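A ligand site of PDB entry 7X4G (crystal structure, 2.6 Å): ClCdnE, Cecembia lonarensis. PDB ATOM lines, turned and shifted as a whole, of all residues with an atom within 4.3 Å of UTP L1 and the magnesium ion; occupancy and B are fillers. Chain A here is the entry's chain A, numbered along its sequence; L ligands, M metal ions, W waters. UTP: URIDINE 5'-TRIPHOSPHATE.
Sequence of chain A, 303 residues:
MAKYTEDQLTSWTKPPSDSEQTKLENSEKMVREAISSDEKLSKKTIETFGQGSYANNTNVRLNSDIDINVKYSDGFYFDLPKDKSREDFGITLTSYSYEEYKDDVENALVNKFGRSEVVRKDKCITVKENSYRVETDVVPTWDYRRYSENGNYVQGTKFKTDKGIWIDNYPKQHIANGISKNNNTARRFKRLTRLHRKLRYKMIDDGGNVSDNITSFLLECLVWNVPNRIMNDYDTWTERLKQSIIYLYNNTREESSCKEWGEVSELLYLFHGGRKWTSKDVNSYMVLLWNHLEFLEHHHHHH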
ATOM      1  N   GLN A  51      26.928   2.733  23.518  1.00  0.00           N
ATOM      2  CA  GLN A  51      26.551   1.451  24.098  1.00  0.00           C
ATOM      3  C   GLN A  51      25.032   1.341  24.085  1.00  0.00           C
ATOM      4  O   GLN A  51      24.336   2.246  23.624  1.00  0.00           O
ATOM      5  CB  GLN A  51      27.117   1.288  25.521  1.00  0.00           C
ATOM      6  CG  GLN A  51      26.621   2.320  26.513  1.00  0.00           C
ATOM      7  CD  GLN A  51      27.159   2.083  27.913  1.00  0.00           C
ATOM      8  OE1 GLN A  51      28.354   1.824  28.092  1.00  0.00           O
ATOM      9  NE2 GLN A  51      26.282   2.171  28.910  1.00  0.00           N
ATOM     10  N   GLY A  52      24.525   0.218  24.574  1.00  0.00           N
ATOM     11  CA  GLY A  52      23.089   0.037  24.641  1.00  0.00           C
ATOM     12  C   GLY A  52      22.436  -0.205  23.283  1.00  0.00           C
ATOM     13  O   GLY A  52      23.073  -0.602  22.306  1.00  0.00           O
ATOM     14  N   SER A  53      21.129   0.075  23.251  1.00  0.00           N
ATOM     15  CA  SER A  53      20.286  -0.407  22.154  1.00  0.00           C
ATOM     16  C   SER A  53      20.649   0.231  20.812  1.00  0.00           C
ATOM     17  O   SER A  53      20.500  -0.415  19.772  1.00  0.00           O
ATOM     18  CB  SER A  53      18.819  -0.138  22.473  1.00  0.00           C
ATOM     19  OG  SER A  53      18.611   1.207  22.878  1.00  0.00           O
ATOM     20  N   ASN A  56      23.844  -1.557  19.654  1.00  0.00           N
ATOM     21  CA  ASN A  56      23.581  -2.944  19.294  1.00  0.00           C
ATOM     22  C   ASN A  56      22.520  -3.053  18.207  1.00  0.00           C
ATOM     23  O   ASN A  56      22.119  -4.172  17.863  1.00  0.00           O
ATOM     24  CB  ASN A  56      23.137  -3.740  20.527  1.00  0.00           C
ATOM     25  CG  ASN A  56      24.253  -3.893  21.554  1.00  0.00           C
ATOM     26  OD1 ASN A  56      25.169  -4.705  21.379  1.00  0.00           O
ATOM     27  ND2 ASN A  56      24.173  -3.111  22.631  1.00  0.00           N
ATOM     28  N   ARG A  61      12.097   1.748  20.090  1.00  0.00           N
ATOM     29  CA  ARG A  61      11.316   2.935  20.403  1.00  0.00           C
ATOM     30  C   ARG A  61      11.922   4.133  19.692  1.00  0.00           C
ATOM     31  O   ARG A  61      13.089   4.458  19.906  1.00  0.00           O
ATOM     32  CB  ARG A  61      11.241   3.181  21.906  1.00  0.00           C
ATOM     33  CG  ARG A  61      10.306   2.234  22.646  1.00  0.00           C
ATOM     34  CD  ARG A  61      10.252   2.553  24.132  1.00  0.00           C
ATOM     35  NE  ARG A  61      11.588   2.560  24.743  1.00  0.00           N
ATOM     36  CZ  ARG A  61      11.844   3.026  25.961  1.00  0.00           C
ATOM     37  NH1 ARG A  61      13.079   2.992  26.436  1.00  0.00           N
ATOM     38  NH2 ARG A  61      10.860   3.534  26.702  1.00  0.00           N
ATOM     39  N   ASP A  65      16.191   7.027  24.429  1.00  0.00           N
ATOM     40  CA  ASP A  65      17.498   7.516  24.862  1.00  0.00           C
ATOM     41  C   ASP A  65      18.622   6.734  24.178  1.00  0.00           C
ATOM     42  O   ASP A  65      18.558   5.514  24.038  1.00  0.00           O
ATOM     43  CB  ASP A  65      17.630   7.412  26.379  1.00  0.00           C
ATOM     44  CG  ASP A  65      16.699   8.351  27.110  1.00  0.00           C
ATOM     45  OD1 ASP A  65      15.873   9.004  26.440  1.00  0.00           O
ATOM     46  OD2 ASP A  65      16.796   8.441  28.355  1.00  0.00           O
ATOM     47  N   ASP A  67      22.573   5.765  24.622  1.00  0.00           N
ATOM     48  CA  ASP A  67      23.574   5.664  25.676  1.00  0.00           C
ATOM     49  C   ASP A  67      24.966   5.877  25.107  1.00  0.00           C
ATOM     50  O   ASP A  67      25.409   5.135  24.231  1.00  0.00           O
ATOM     51  CB  ASP A  67      23.486   4.297  26.362  1.00  0.00           C
ATOM     52  CG  ASP A  67      22.073   3.985  26.841  1.00  0.00           C
ATOM     53  OD1 ASP A  67      21.492   4.826  27.549  1.00  0.00           O
ATOM     54  OD2 ASP A  67      21.556   2.898  26.499  1.00  0.00           O
ATOM     55  N   ASN A 169      30.804  -3.235  33.938  1.00  0.00           N
ATOM     56  CA  ASN A 169      30.148  -3.541  32.677  1.00  0.00           C
ATOM     57  C   ASN A 169      31.191  -3.980  31.653  1.00  0.00           C
ATOM     58  O   ASN A 169      32.386  -3.714  31.799  1.00  0.00           O
ATOM     59  CB  ASN A 169      29.396  -2.312  32.127  1.00  0.00           C
ATOM     60  CG  ASN A 169      28.094  -2.040  32.849  1.00  0.00           C
ATOM     61  OD1 ASN A 169      27.504  -0.969  32.709  1.00  0.00           O
ATOM     62  ND2 ASN A 169      27.628  -3.012  33.631  1.00  0.00           N
ATOM     63  N   PRO A 171      30.709  -3.406  27.850  1.00  0.00           N
ATOM     64  CA  PRO A 171      29.888  -3.035  26.681  1.00  0.00           C
ATOM     65  C   PRO A 171      30.503  -3.422  25.352  1.00  0.00           C
ATOM     66  O   PRO A 171      29.783  -3.813  24.429  1.00  0.00           O
ATOM     67  CB  PRO A 171      29.742  -1.511  26.829  1.00  0.00           C
ATOM     68  CG  PRO A 171      30.943  -1.096  27.608  1.00  0.00           C
ATOM     69  CD  PRO A 171      31.253  -2.224  28.550  1.00  0.00           C
ATOM     70  N   HIS A 174      30.024  -7.012  24.766  1.00  0.00           N
ATOM     71  CA  HIS A 174      28.591  -7.156  24.526  1.00  0.00           C
ATOM     72  C   HIS A 174      28.267  -6.911  23.065  1.00  0.00           C
ATOM     73  O   HIS A 174      27.621  -7.744  22.403  1.00  0.00           O
ATOM     74  CB  HIS A 174      27.832  -6.199  25.450  1.00  0.00           C
ATOM     75  CG  HIS A 174      26.342  -6.234  25.307  1.00  0.00           C
ATOM     76  ND1 HIS A 174      25.502  -6.383  26.401  1.00  0.00           N
ATOM     77  CD2 HIS A 174      25.532  -6.118  24.230  1.00  0.00           C
ATOM     78  CE1 HIS A 174      24.244  -6.373  25.993  1.00  0.00           C
ATOM     79  NE2 HIS A 174      24.240  -6.216  24.681  1.00  0.00           N
ATOM     80  N   ARG A 197      11.460  -7.026  22.654  1.00  0.00           N
ATOM     81  CA  ARG A 197      11.377  -5.712  23.285  1.00  0.00           C
ATOM     82  C   ARG A 197      10.051  -5.040  22.985  1.00  0.00           C
ATOM     83  O   ARG A 197       9.364  -4.512  23.879  1.00  0.00           O
ATOM     84  CB  ARG A 197      12.542  -4.835  22.822  1.00  0.00           C
ATOM     85  CG  ARG A 197      13.895  -5.212  23.391  1.00  0.00           C
ATOM     86  CD  ARG A 197      15.007  -4.571  22.572  1.00  0.00           C
ATOM     87  NE  ARG A 197      16.321  -4.709  23.207  1.00  0.00           N
ATOM     88  CZ  ARG A 197      16.975  -3.705  23.787  1.00  0.00           C
ATOM     89  NH1 ARG A 197      16.435  -2.503  23.832  1.00  0.00           N
ATOM     90  NH2 ARG A 197      18.166  -3.913  24.334  1.00  0.00           N
ATOM     91  N   TYR A 201       6.884  -3.922  25.466  1.00  0.00           N
ATOM     92  CA  TYR A 201       6.296  -2.588  25.531  1.00  0.00           C
ATOM     93  C   TYR A 201       4.787  -2.637  25.288  1.00  0.00           C
ATOM     94  O   TYR A 201       4.033  -1.955  25.989  1.00  0.00           O
ATOM     95  CB  TYR A 201       6.990  -1.663  24.526  1.00  0.00           C
ATOM     96  CG  TYR A 201       8.364  -1.235  24.975  1.00  0.00           C
ATOM     97  CD1 TYR A 201       8.567  -0.694  26.246  1.00  0.00           C
ATOM     98  CD2 TYR A 201       9.480  -1.376  24.148  1.00  0.00           C
ATOM     99  CE1 TYR A 201       9.814  -0.298  26.670  1.00  0.00           C
ATOM    100  CE2 TYR A 201      10.741  -0.985  24.563  1.00  0.00           C
ATOM    101  CZ  TYR A 201      10.908  -0.446  25.824  1.00  0.00           C
ATOM    102  OH  TYR A 201      12.155  -0.050  26.248  1.00  0.00           O
ATOM    103  N   SER A 216      15.033  -4.166  29.499  1.00  0.00           N
ATOM    104  CA  SER A 216      15.382  -4.382  28.105  1.00  0.00           C
ATOM    105  C   SER A 216      16.716  -5.105  27.975  1.00  0.00           C
ATOM    106  O   SER A 216      16.876  -5.994  27.141  1.00  0.00           O
ATOM    107  CB  SER A 216      15.432  -3.044  27.353  1.00  0.00           C
ATOM    108  OG  SER A 216      14.155  -2.715  26.838  1.00  0.00           O
ATOM    109  N   PHE A 217      17.701  -4.716  28.799  1.00  0.00           N
ATOM    110  CA  PHE A 217      18.969  -5.428  28.850  1.00  0.00           C
ATOM    111  C   PHE A 217      18.765  -6.901  29.180  1.00  0.00           C
ATOM    112  O   PHE A 217      19.417  -7.785  28.597  1.00  0.00           O
ATOM    113  CB  PHE A 217      19.894  -4.758  29.874  1.00  0.00           C
ATOM    114  CG  PHE A 217      21.163  -5.512  30.152  1.00  0.00           C
ATOM    115  CD1 PHE A 217      22.302  -5.283  29.401  1.00  0.00           C
ATOM    116  CD2 PHE A 217      21.226  -6.426  31.194  1.00  0.00           C
ATOM    117  CE1 PHE A 217      23.470  -5.960  29.669  1.00  0.00           C
ATOM    118  CE2 PHE A 217      22.386  -7.108  31.463  1.00  0.00           C
ATOM    119  CZ  PHE A 217      23.519  -6.874  30.701  1.00  0.00           C
ATOM    120  N   ARG A 275      21.695  -8.940  40.778  1.00  0.00           N
ATOM    121  CA  ARG A 275      20.786  -8.580  39.704  1.00  0.00           C
ATOM    122  C   ARG A 275      19.419  -8.240  40.285  1.00  0.00           C
ATOM    123  O   ARG A 275      19.001  -8.811  41.301  1.00  0.00           O
ATOM    124  CB  ARG A 275      20.651  -9.719  38.689  1.00  0.00           C
ATOM    125  CG  ARG A 275      21.974 -10.212  38.114  1.00  0.00           C
ATOM    126  CD  ARG A 275      22.701  -9.116  37.356  1.00  0.00           C
ATOM    127  NE  ARG A 275      23.577  -9.671  36.327  1.00  0.00           N
ATOM    128  CZ  ARG A 275      24.105  -8.969  35.333  1.00  0.00           C
ATOM    129  NH1 ARG A 275      23.839  -7.669  35.214  1.00  0.00           N
ATOM    130  NH2 ARG A 275      24.903  -9.554  34.454  1.00  0.00           N
ATOM    131  N   TRP A 277      16.700  -8.969  38.915  1.00  0.00           N
ATOM    132  CA  TRP A 277      15.787 -10.009  38.464  1.00  0.00           C
ATOM    133  C   TRP A 277      16.190 -11.360  39.049  1.00  0.00           C
ATOM    134  O   TRP A 277      17.230 -11.500  39.691  1.00  0.00           O
ATOM    135  CB  TRP A 277      15.759 -10.086  36.929  1.00  0.00           C
ATOM    136  CG  TRP A 277      17.118 -10.252  36.327  1.00  0.00           C
ATOM    137  CD1 TRP A 277      17.819 -11.425  36.194  1.00  0.00           C
ATOM    138  CD2 TRP A 277      17.942  -9.226  35.762  1.00  0.00           C
ATOM    139  NE1 TRP A 277      19.031 -11.185  35.586  1.00  0.00           N
ATOM    140  CE2 TRP A 277      19.134  -9.842  35.307  1.00  0.00           C
ATOM    141  CE3 TRP A 277      17.795  -7.844  35.595  1.00  0.00           C
ATOM    142  CZ2 TRP A 277      20.161  -9.133  34.708  1.00  0.00           C
ATOM    143  CZ3 TRP A 277      18.821  -7.137  34.985  1.00  0.00           C
ATOM    144  CH2 TRP A 277      19.986  -7.778  34.556  1.00  0.00           C
HETATM  145  PA  UTP L   1      20.312   0.071  29.073  1.00  0.00           P
HETATM  146  O1A UTP L   1      19.609  -0.132  30.368  1.00  0.00           O
HETATM  147  O2A UTP L   1      19.879   1.401  28.441  1.00  0.00           O
HETATM  148  O3A UTP L   1      19.961  -1.184  28.042  1.00  0.00           O
HETATM  149  O5' UTP L   1      21.957   0.079  29.327  1.00  0.00           O
HETATM  150  PB  UTP L   1      19.397  -0.976  26.495  1.00  0.00           P
HETATM  151  O1B UTP L   1      19.976   0.308  25.907  1.00  0.00           O
HETATM  152  O2B UTP L   1      19.817  -2.172  25.655  1.00  0.00           O
HETATM  153  O3B UTP L   1      17.743  -0.907  26.531  1.00  0.00           O
HETATM  154  PG  UTP L   1      16.891   0.491  26.638  1.00  0.00           P
HETATM  155  O1G UTP L   1      15.837   0.530  25.526  1.00  0.00           O
HETATM  156  O2G UTP L   1      16.216   0.567  27.980  1.00  0.00           O
HETATM  157  O3G UTP L   1      17.829   1.671  26.480  1.00  0.00           O
HETATM  158  C5' UTP L   1      22.803   0.252  28.216  1.00  0.00           C
HETATM  159  C4' UTP L   1      24.067  -0.592  28.392  1.00  0.00           C
HETATM  160  O4' UTP L   1      24.576  -0.543  29.878  1.00  0.00           O
HETATM  161  C1' UTP L   1      25.096  -1.968  30.184  1.00  0.00           C
HETATM  162  C2' UTP L   1      24.970  -2.637  29.036  1.00  0.00           C
HETATM  163  O2' UTP L   1      26.210  -2.595  28.301  1.00  0.00           O
HETATM  164  C3' UTP L   1      23.816  -1.867  28.201  1.00  0.00           C
HETATM  165  O3' UTP L   1      23.905  -2.204  26.791  1.00  0.00           O
HETATM  166  N1  UTP L   1      24.303  -2.599  31.251  1.00  0.00           N
HETATM  167  C6  UTP L   1      23.099  -2.128  31.555  1.00  0.00           C
HETATM  168  C2  UTP L   1      24.804  -3.676  31.915  1.00  0.00           C
HETATM  169  O2  UTP L   1      25.896  -4.118  31.643  1.00  0.00           O
HETATM  170  N3  UTP L   1      24.067  -4.264  32.901  1.00  0.00           N
HETATM  171  C4  UTP L   1      22.868  -3.801  33.207  1.00  0.00           C
HETATM  172  O4  UTP L   1      22.224  -4.317  34.074  1.00  0.00           O
HETATM  173  C5  UTP L   1      22.362  -2.715  32.541  1.00  0.00           C
HETATM  174  PA  UTP L   2      18.802   2.438  34.432  1.00  0.00           P
HETATM  175  O1A UTP L   2      19.484   1.072  34.376  1.00  0.00           O
HETATM  176  O2A UTP L   2      17.326   2.253  34.294  1.00  0.00           O
HETATM  177  O3A UTP L   2      19.166   3.161  35.888  1.00  0.00           O
HETATM  178  O5' UTP L   2      19.332   3.376  33.186  1.00  0.00           O
HETATM  179  PB  UTP L   2      18.111   4.100  36.761  1.00  0.00           P
HETATM  180  O1B UTP L   2      17.055   4.680  35.839  1.00  0.00           O
HETATM  181  O2B UTP L   2      18.869   5.227  37.447  1.00  0.00           O
HETATM  182  O3B UTP L   2      17.400   3.122  37.902  1.00  0.00           O
HETATM  183  PG  UTP L   2      15.972   2.341  37.732  1.00  0.00           P
HETATM  184  O1G UTP L   2      15.521   2.382  36.298  1.00  0.00           O
HETATM  185  O2G UTP L   2      16.144   0.902  38.151  1.00  0.00           O
HETATM  186  O3G UTP L   2      14.913   2.994  38.612  1.00  0.00           O
HETATM  187  C5' UTP L   2      20.286   4.386  33.449  1.00  0.00           C
HETATM  188  C4' UTP L   2      21.264   4.436  32.277  1.00  0.00           C
HETATM  189  O4' UTP L   2      22.718   4.253  32.842  1.00  0.00           O
HETATM  190  C1' UTP L   2      23.399   3.231  31.922  1.00  0.00           C
HETATM  191  C2' UTP L   2      22.531   2.961  30.948  1.00  0.00           C
HETATM  192  O2' UTP L   2      22.878   3.714  29.764  1.00  0.00           O
HETATM  193  C3' UTP L   2      21.067   3.421  31.479  1.00  0.00           C
HETATM  194  O3' UTP L   2      20.211   3.782  30.364  1.00  0.00           O
HETATM  195  N1  UTP L   2      23.775   2.012  32.661  1.00  0.00           N
HETATM  196  C6  UTP L   2      22.939   1.436  33.518  1.00  0.00           C
HETATM  197  C2  UTP L   2      25.003   1.470  32.455  1.00  0.00           C
HETATM  198  O2  UTP L   2      25.774   1.994  31.671  1.00  0.00           O
HETATM  199  N3  UTP L   2      25.379   0.344  33.120  1.00  0.00           N
HETATM  200  C4  UTP L   2      24.544  -0.232  33.978  1.00  0.00           C
HETATM  201  O4  UTP L   2      24.870  -1.225  34.569  1.00  0.00           O
HETATM  202  C5  UTP L   2      23.302   0.312  34.182  1.00  0.00           C
HETATM  203 MG    MG M   1      19.686   2.300  26.599  1.00  0.00          MG
HETATM  204  O   HOH W   1      22.961  -5.698  37.159  1.00  0.00           O
HETATM  205  O   HOH W   2      13.792  -1.659  24.699  1.00  0.00           O
HETATM  206  O   HOH W   3      14.810   2.325  29.383  1.00  0.00           O
HETATM  207  O   HOH W   4      26.274  -2.378  25.237  1.00  0.00           O
HETATM  208  O   HOH W   5      14.596   0.581  22.836  1.00  0.00           O
HETATM  209  O   HOH W   6      17.060   1.934  30.593  1.00  0.00           O
HETATM  210  O   HOH W   7      16.437   3.745  25.165  1.00  0.00           O
HETATM  211  O   HOH W   8      19.656   2.991  24.613  1.00  0.00           O
HETATM  212  O   HOH W   9      27.437  -4.686  28.404  1.00  0.00           O
HETATM  213  O   HOH W  10      19.129   4.107  27.435  1.00  0.00           O
HETATM  214  O   HOH W  11      17.580  -2.046  30.400  1.00  0.00           O
HETATM  215  O   HOH W  12      21.282  -3.182  23.549  1.00  0.00           O
HETATM  216  O   HOH W  13      21.846  -3.829  26.425  1.00  0.00           O
HETATM  217  O   HOH W  14      25.897  -6.335  33.757  1.00  0.00           O
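One residue has an atom within 4 Å of the magnesium ion: Asp 67.
Residues that only touch UTP L1: Ser 216 (3.3 Å), Phe 217 (3.5 Å), Tyr 201 (3.8 Å), Arg 275 (3.9 Å) and Pro 171 (3.98 Å).
Within 4 Å of UTP L1: Gln 51, Gly 52, Ser 53, Arg 61, Asp 67, Asn 169, Pro 171, Arg 197, Tyr 201, Ser 216, Phe 217 and Arg 275.
Along chain A the residues within 4 Å of UTP L1 span positions 51 to 275.
The nearest printed residue that does not touch UTP L1 is Trp 277 (4.1 Å).
The backbone carbonyl oxygen of Asp 67 sits at hydrogen-bond distance from the backbone NH of Gln 51 (2.9 Å).
The side-chain amide nitrogen of Asn 56 sits at hydrogen-bond distance from the backbone carbonyl oxygen of Gly 52, at 2.8 Å.
OH of Tyr 201 sits at hydrogen-bond distance from OG of Ser 216.
The guanidinium group of Arg 61 lies within hydrogen-bond range of the side-chain hydroxyl of Tyr 201 (3.1 Å).
The guanidinium group (NH2) of Arg 197 lies within salt-bridge range of an oxygen (O2B) of UTP L1.
The side-chain amide nitrogen (ND2) of Asn 169 is in hydrogen-bond range of an oxygen (O2) of UTP L1 (2.9 Å).
N of Ser 53 sits close to O1B of UTP L1, at 2.9 Å.
An oxygen (O1B) of UTP L1 lies close to the side-chain hydroxyl (OG) of Ser 53 (3.4 Å).
The backbone NH (N) of Gly 52 sits close to an oxygen (O3') of UTP L1.
NE2 of Gln 51 is in hydrogen-bond range of O4' of UTP L1, at 3.3 Å.
An oxygen (O1G) of UTP L1 lies within salt-bridge range of the guanidinium group of Arg 61, at 3.8 Å.
OD1 of Asp 67 sits at hydrogen-bond distance from O2' of UTP L2 (2.8 Å).
OD1 of Asn 169 sits at hydrogen-bond distance from N3 of UTP L2 (2.5 Å).
An oxygen (O2) of UTP L2 sits at hydrogen-bond distance from the side-chain amide nitrogen (NE2) of Gln 51, at 2.8 Å.
Water W8 bridges OG of Ser 53 (2.7 Å) and O of Asp 65 (2.8 Å).
Water W9 lies within hydrogen-bond range of O2' of UTP L1 (2.4 Å) and ND1 of His 174 (3.3 Å).
Water W11 lies within hydrogen-bond range of O1A of UTP L1 (2.8 Å), N of Phe 217 (3.1 Å) and N of Ser 216 (3.4 Å).
Water W4 lies within hydrogen-bond range of an oxygen (O3') of UTP L1 (2.8 Å), the backbone NH (N) of Gly 52 (3.2 Å) and the side-chain amide nitrogen (ND2) of Asn 56 (3.4 Å).
Water W14 lies within hydrogen-bond range of the guanidinium group of Arg 275 and a nitrogen (N3) of UTP L1.
Water W1 bridges the guanidinium group of Arg 275 (2.9 Å) and an oxygen (O4) of UTP L1 (3.5 Å).
The magnesium ion is bound by an oxygen (O3G) of UTP L1 (2.0 Å), the side-chain carboxylate of Asp 67 (2.0 Å), an oxygen (O2A) of UTP L1 (2.1 Å), water W10 (2.1 Å), water W8 (2.1 Å) and an oxygen (O1B) of UTP L1 (2.1 Å).
N3 of UTP L2 lies close to O4' of UTP L1, at 3.5 Å.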
